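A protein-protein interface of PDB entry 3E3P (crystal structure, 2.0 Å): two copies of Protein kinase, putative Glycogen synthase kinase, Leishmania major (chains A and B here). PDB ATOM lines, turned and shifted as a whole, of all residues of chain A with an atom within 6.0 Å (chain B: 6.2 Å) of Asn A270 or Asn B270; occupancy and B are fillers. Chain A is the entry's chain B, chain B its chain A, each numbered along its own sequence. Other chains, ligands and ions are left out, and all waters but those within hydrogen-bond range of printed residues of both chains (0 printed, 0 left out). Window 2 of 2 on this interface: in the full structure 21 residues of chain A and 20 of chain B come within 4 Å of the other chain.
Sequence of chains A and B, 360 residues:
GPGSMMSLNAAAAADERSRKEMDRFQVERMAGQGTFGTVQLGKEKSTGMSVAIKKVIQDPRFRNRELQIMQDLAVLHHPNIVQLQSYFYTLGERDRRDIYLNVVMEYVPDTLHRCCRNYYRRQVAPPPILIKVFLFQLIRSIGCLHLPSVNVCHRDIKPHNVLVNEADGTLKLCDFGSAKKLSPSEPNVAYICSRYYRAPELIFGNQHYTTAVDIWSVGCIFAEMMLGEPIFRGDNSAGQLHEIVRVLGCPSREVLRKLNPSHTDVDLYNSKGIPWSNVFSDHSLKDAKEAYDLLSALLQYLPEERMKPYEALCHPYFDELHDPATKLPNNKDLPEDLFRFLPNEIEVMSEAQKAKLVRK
O of Asp B267 lies within hydrogen-bond range of N of Asn A270, at 2.9 Å.
The backbone NH (N) of Tyr B269 is in hydrogen-bond range of the backbone carbonyl oxygen (O) of Leu A268, 3.4 Å away.
ND2 of Asn B270 lies within hydrogen-bond range of O of Asp A267 (3.0 Å).
N of Asn B270 is in hydrogen-bond range of O of Leu A268 (3.0 Å).
The backbone carbonyl oxygen of Leu A268 lies close to the backbone carbonyl oxygen of Asp B267 (3.5 Å).
O of Leu A268 sits close to O of Leu B268 (3.2 Å).
SG of Cys B250 sits close to O of Tyr B269 (3.3 Å).
The side-chain hydroxyl (OG) of Ser A271 is in hydrogen-bond range of the backbone carbonyl oxygen (O) of Val A245.
N of Cys A250 sits at hydrogen-bond distance from O of Ser A271, 2.9 Å away.
Among the printed residues, pairs that only touch across the chains: Asn A270 with Asn B270 (3.7 Å), Val A245 with Leu B268 (3.7 Å) and Ser A271 with Leu B268 (3.8 Å).
Printed residues of chain B within 4 Å of Asn A270: Asp B267 and Asn B270.
Of chain A, only Asp A267, Leu A268 and Asn A270 come within 4 Å of Asn B270.
Printed residues of chain B within 4 Å of Val A245: Leu B268 (3.7 Å).
Printed residues of chain A within 4 Å of Leu B268: Val A245 (3.7 Å), Leu A268 (3.0 Å) and Ser A271 (3.8 Å).
Of the printed residues of chain B, Asp A267 touches Asn B270 (3.0 Å).
Of the printed residues of chain A, Asp B267 touches Leu A268 (3.5 Å) and Asn A270 (2.9 Å).
Printed residues of chain B within 4 Å of Leu A268: Asp B267, Leu B268, Tyr B269 and Asn B270.
Cys A250 touches none of the printed residues of chain B.
Lys B272 touches none of the printed residues of chain A.
The nearest residue of chain B that does not touch Asn A270 is Leu B268 (4.4 Å).
The nearest residue of chain A that does not touch Asn B270 is Tyr A269 (5.1 Å).
The nearest printed residue of chain A that does not touch Leu B268 is Tyr A269 (4.4 Å).
Of the 9 printed residues of chain A, 5 touch a printed residue of chain B.
Hydrophobic or aromatic side chains of chain B within 4 Å of the printed part of chain A: Leu B268.
Along chain B the printed residues that touch a printed residue of chain A span positions 267 to 270.
Among the printed residues, 9 pairs touch across the chains.
Among the printed residues, no Asp or Glu carboxylate lies within 4 Å of a Lys or Arg side-chain nitrogen of the other chain.
Asp A267 touches Asn B270, and with the chains exchanged Asn A270 touches Asp B267.
Leu A268 touches its own counterpart, Leu B268.
Leu A268 touches Asn B270, but with the chains exchanged Asn A270 does not touch Leu B268 (4.4 Å).
Asn A270 touches its own counterpart, Asn B270.
Positions printed for both chains: 245, 250, 266, 267, 268, 269, 270, 271 and 272.
Of the 9 pairs that touch across the chains among the printed residues, 4 have their exchanged pair printed and touching as well.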
ATOM      1  N   VAL A 245     -18.716   8.636 -23.600  1.00  0.00           N
ATOM      2  CA  VAL A 245     -19.124   9.986 -24.025  1.00  0.00           C
ATOM      3  C   VAL A 245     -19.391  10.921 -22.837  1.00  0.00           C
ATOM      4  O   VAL A 245     -19.009  12.107 -22.859  1.00  0.00           O
ATOM      5  CB  VAL A 245     -20.381   9.937 -24.923  1.00  0.00           C
ATOM      6  CG1 VAL A 245     -20.950  11.344 -25.167  1.00  0.00           C
ATOM      7  CG2 VAL A 245     -20.060   9.258 -26.234  1.00  0.00           C
ATOM      8  N   CYS A 250     -18.683  14.566 -26.586  1.00  0.00           N
ATOM      9  CA  CYS A 250     -19.103  14.170 -27.925  1.00  0.00           C
ATOM     10  C   CYS A 250     -17.894  13.901 -28.821  1.00  0.00           C
ATOM     11  O   CYS A 250     -16.941  14.687 -28.829  1.00  0.00           O
ATOM     12  CB  CYS A 250     -19.975  15.251 -28.567  1.00  0.00           C
ATOM     13  SG  CYS A 250     -20.766  14.692 -30.119  1.00  0.00           S
ATOM     14  N   VAL A 266     -23.788  14.086 -34.798  1.00  0.00           N
ATOM     15  CA  VAL A 266     -23.147  14.418 -33.510  1.00  0.00           C
ATOM     16  C   VAL A 266     -24.116  15.008 -32.496  1.00  0.00           C
ATOM     17  O   VAL A 266     -23.831  15.001 -31.303  1.00  0.00           O
ATOM     18  CB  VAL A 266     -21.950  15.411 -33.670  1.00  0.00           C
ATOM     19  CG1 VAL A 266     -20.937  14.893 -34.694  1.00  0.00           C
ATOM     20  CG2 VAL A 266     -22.442  16.813 -34.049  1.00  0.00           C
ATOM     21  N   ASP A 267     -25.252  15.519 -32.972  1.00  0.00           N
ATOM     22  CA  ASP A 267     -26.252  16.157 -32.100  1.00  0.00           C
ATOM     23  C   ASP A 267     -26.798  15.222 -31.025  1.00  0.00           C
ATOM     24  O   ASP A 267     -27.173  15.680 -29.947  1.00  0.00           O
ATOM     25  CB  ASP A 267     -27.436  16.707 -32.919  1.00  0.00           C
ATOM     26  CG  ASP A 267     -27.050  17.887 -33.812  1.00  0.00           C
ATOM     27  OD1 ASP A 267     -25.989  18.518 -33.585  1.00  0.00           O
ATOM     28  OD2 ASP A 267     -27.825  18.189 -34.750  1.00  0.00           O
ATOM     29  N   LEU A 268     -26.849  13.924 -31.323  1.00  0.00           N
ATOM     30  CA  LEU A 268     -27.369  12.939 -30.372  1.00  0.00           C
ATOM     31  C   LEU A 268     -26.516  12.863 -29.098  1.00  0.00           C
ATOM     32  O   LEU A 268     -27.037  12.645 -28.000  1.00  0.00           O
ATOM     33  CB  LEU A 268     -27.516  11.557 -31.034  1.00  0.00           C
ATOM     34  CG  LEU A 268     -28.828  11.387 -31.819  1.00  0.00           C
ATOM     35  CD1 LEU A 268     -28.914  12.369 -32.984  1.00  0.00           C
ATOM     36  CD2 LEU A 268     -29.011   9.950 -32.314  1.00  0.00           C
ATOM     37  N   TYR A 269     -25.217  13.088 -29.253  1.00  0.00           N
ATOM     38  CA  TYR A 269     -24.274  13.056 -28.143  1.00  0.00           C
ATOM     39  C   TYR A 269     -23.989  14.467 -27.607  1.00  0.00           C
ATOM     40  O   TYR A 269     -22.870  14.967 -27.741  1.00  0.00           O
ATOM     41  CB  TYR A 269     -22.974  12.397 -28.611  1.00  0.00           C
ATOM     42  CG  TYR A 269     -23.195  11.109 -29.366  1.00  0.00           C
ATOM     43  CD1 TYR A 269     -23.790  10.014 -28.742  1.00  0.00           C
ATOM     44  CD2 TYR A 269     -22.812  10.983 -30.701  1.00  0.00           C
ATOM     45  CE1 TYR A 269     -24.003   8.819 -29.425  1.00  0.00           C
ATOM     46  CE2 TYR A 269     -23.020   9.789 -31.402  1.00  0.00           C
ATOM     47  CZ  TYR A 269     -23.619   8.708 -30.755  1.00  0.00           C
ATOM     48  OH  TYR A 269     -23.836   7.519 -31.418  1.00  0.00           O
ATOM     49  N   ASN A 270     -24.995  15.101 -27.002  1.00  0.00           N
ATOM     50  CA  ASN A 270     -24.853  16.472 -26.487  1.00  0.00           C
ATOM     51  C   ASN A 270     -24.177  16.508 -25.102  1.00  0.00           C
ATOM     52  O   ASN A 270     -24.816  16.799 -24.084  1.00  0.00           O
ATOM     53  CB  ASN A 270     -26.219  17.179 -26.443  1.00  0.00           C
ATOM     54  CG  ASN A 270     -26.111  18.653 -26.084  1.00  0.00           C
ATOM     55  OD1 ASN A 270     -25.179  19.341 -26.501  1.00  0.00           O
ATOM     56  ND2 ASN A 270     -27.073  19.146 -25.312  1.00  0.00           N
ATOM     57  N   SER A 271     -22.876  16.216 -25.085  1.00  0.00           N
ATOM     58  CA  SER A 271     -22.098  16.153 -23.851  1.00  0.00           C
ATOM     59  C   SER A 271     -20.756  16.831 -24.026  1.00  0.00           C
ATOM     60  O   SER A 271     -20.031  16.546 -24.979  1.00  0.00           O
ATOM     61  CB  SER A 271     -21.882  14.693 -23.432  1.00  0.00           C
ATOM     62  OG  SER A 271     -20.778  14.565 -22.545  1.00  0.00           O
ATOM     63  N   LYS A 272     -20.431  17.718 -23.090  1.00  0.00           N
ATOM     64  CA  LYS A 272     -19.128  18.394 -23.062  1.00  0.00           C
ATOM     65  C   LYS A 272     -18.052  17.566 -22.336  1.00  0.00           C
ATOM     66  O   LYS A 272     -16.870  17.921 -22.353  1.00  0.00           O
ATOM     67  CB  LYS A 272     -19.256  19.777 -22.392  1.00  0.00           C
ATOM     68  CG  LYS A 272     -19.829  19.762 -20.948  1.00  0.00           C
ATOM     69  CD  LYS A 272     -19.407  21.013 -20.135  1.00  0.00           C
ATOM     70  CE  LYS A 272     -20.014  21.035 -18.732  1.00  0.00           C
ATOM     71  NZ  LYS A 272     -21.511  20.919 -18.740  1.00  0.00           N
ATOM     72  N   VAL B 245     -33.402   6.642 -32.054  1.00  0.00           N
ATOM     73  CA  VAL B 245     -33.447   7.943 -31.355  1.00  0.00           C
ATOM     74  C   VAL B 245     -33.500   9.079 -32.371  1.00  0.00           C
ATOM     75  O   VAL B 245     -34.261  10.037 -32.214  1.00  0.00           O
ATOM     76  CB  VAL B 245     -32.235   8.133 -30.401  1.00  0.00           C
ATOM     77  CG1 VAL B 245     -32.194   9.548 -29.857  1.00  0.00           C
ATOM     78  CG2 VAL B 245     -32.313   7.153 -29.264  1.00  0.00           C
ATOM     79  N   CYS B 250     -35.583  11.682 -28.294  1.00  0.00           N
ATOM     80  CA  CYS B 250     -35.107  11.263 -26.981  1.00  0.00           C
ATOM     81  C   CYS B 250     -36.188  10.513 -26.190  1.00  0.00           C
ATOM     82  O   CYS B 250     -37.332  10.981 -26.104  1.00  0.00           O
ATOM     83  CB  CYS B 250     -34.674  12.470 -26.153  1.00  0.00           C
ATOM     84  SG  CYS B 250     -34.014  11.996 -24.523  1.00  0.00           S
ATOM     85  N   VAL B 266     -30.245  12.059 -20.338  1.00  0.00           N
ATOM     86  CA  VAL B 266     -31.065  12.489 -21.478  1.00  0.00           C
ATOM     87  C   VAL B 266     -30.327  13.338 -22.534  1.00  0.00           C
ATOM     88  O   VAL B 266     -30.729  13.354 -23.698  1.00  0.00           O
ATOM     89  CB  VAL B 266     -32.353  13.201 -20.956  1.00  0.00           C
ATOM     90  CG1 VAL B 266     -33.058  13.995 -22.046  1.00  0.00           C
ATOM     91  CG2 VAL B 266     -33.296  12.167 -20.343  1.00  0.00           C
ATOM     92  N   ASP B 267     -29.244  14.008 -22.149  1.00  0.00           N
ATOM     93  CA  ASP B 267     -28.458  14.817 -23.097  1.00  0.00           C
ATOM     94  C   ASP B 267     -27.583  13.996 -24.056  1.00  0.00           C
ATOM     95  O   ASP B 267     -27.096  14.525 -25.059  1.00  0.00           O
ATOM     96  CB  ASP B 267     -27.606  15.841 -22.343  1.00  0.00           C
ATOM     97  CG  ASP B 267     -28.452  16.867 -21.601  1.00  0.00           C
ATOM     98  OD1 ASP B 267     -29.668  16.952 -21.882  1.00  0.00           O
ATOM     99  OD2 ASP B 267     -27.901  17.588 -20.739  1.00  0.00           O
ATOM    100  N   LEU B 268     -27.396  12.711 -23.754  1.00  0.00           N
ATOM    101  CA  LEU B 268     -26.713  11.789 -24.668  1.00  0.00           C
ATOM    102  C   LEU B 268     -27.709  10.984 -25.538  1.00  0.00           C
ATOM    103  O   LEU B 268     -27.333   9.994 -26.183  1.00  0.00           O
ATOM    104  CB  LEU B 268     -25.772  10.857 -23.893  1.00  0.00           C
ATOM    105  CG  LEU B 268     -24.499  11.491 -23.318  1.00  0.00           C
ATOM    106  CD1 LEU B 268     -24.821  12.532 -22.252  1.00  0.00           C
ATOM    107  CD2 LEU B 268     -23.584  10.407 -22.751  1.00  0.00           C
ATOM    108  N   TYR B 269     -28.977  11.407 -25.538  1.00  0.00           N
ATOM    109  CA  TYR B 269     -30.001  10.910 -26.470  1.00  0.00           C
ATOM    110  C   TYR B 269     -30.726  12.126 -27.063  1.00  0.00           C
ATOM    111  O   TYR B 269     -31.959  12.141 -27.161  1.00  0.00           O
ATOM    112  CB  TYR B 269     -31.032  10.017 -25.765  1.00  0.00           C
ATOM    113  CG  TYR B 269     -30.480   8.879 -24.939  1.00  0.00           C
ATOM    114  CD1 TYR B 269     -29.956   7.731 -25.543  1.00  0.00           C
ATOM    115  CD2 TYR B 269     -30.523   8.927 -23.548  1.00  0.00           C
ATOM    116  CE1 TYR B 269     -29.463   6.673 -24.774  1.00  0.00           C
ATOM    117  CE2 TYR B 269     -30.035   7.880 -22.772  1.00  0.00           C
ATOM    118  CZ  TYR B 269     -29.507   6.757 -23.384  1.00  0.00           C
ATOM    119  OH  TYR B 269     -29.027   5.731 -22.596  1.00  0.00           O
ATOM    120  N   ASN B 270     -29.952  13.135 -27.459  1.00  0.00           N
ATOM    121  CA  ASN B 270     -30.491  14.453 -27.813  1.00  0.00           C
ATOM    122  C   ASN B 270     -30.989  14.608 -29.268  1.00  0.00           C
ATOM    123  O   ASN B 270     -30.198  14.882 -30.173  1.00  0.00           O
ATOM    124  CB  ASN B 270     -29.428  15.512 -27.498  1.00  0.00           C
ATOM    125  CG  ASN B 270     -29.871  16.920 -27.853  1.00  0.00           C
ATOM    126  OD1 ASN B 270     -30.891  17.409 -27.357  1.00  0.00           O
ATOM    127  ND2 ASN B 270     -29.093  17.589 -28.705  1.00  0.00           N
ATOM    128  N   SER B 271     -32.294  14.422 -29.486  1.00  0.00           N
ATOM    129  CA  SER B 271     -32.927  14.794 -30.765  1.00  0.00           C
ATOM    130  C   SER B 271     -34.422  15.054 -30.600  1.00  0.00           C
ATOM    131  O   SER B 271     -35.043  14.602 -29.638  1.00  0.00           O
ATOM    132  CB  SER B 271     -32.663  13.771 -31.898  1.00  0.00           C
ATOM    133  OG  SER B 271     -33.545  12.655 -31.884  1.00  0.00           O
ATOM    134  N   LYS B 272     -34.966  15.825 -31.540  1.00  0.00           N
ATOM    135  CA  LYS B 272     -36.391  16.139 -31.576  1.00  0.00           C
ATOM    136  C   LYS B 272     -37.137  14.996 -32.267  1.00  0.00           C
ATOM    137  O   LYS B 272     -38.303  14.733 -31.979  1.00  0.00           O
ATOM    138  CB  LYS B 272     -36.629  17.463 -32.312  1.00  0.00           C
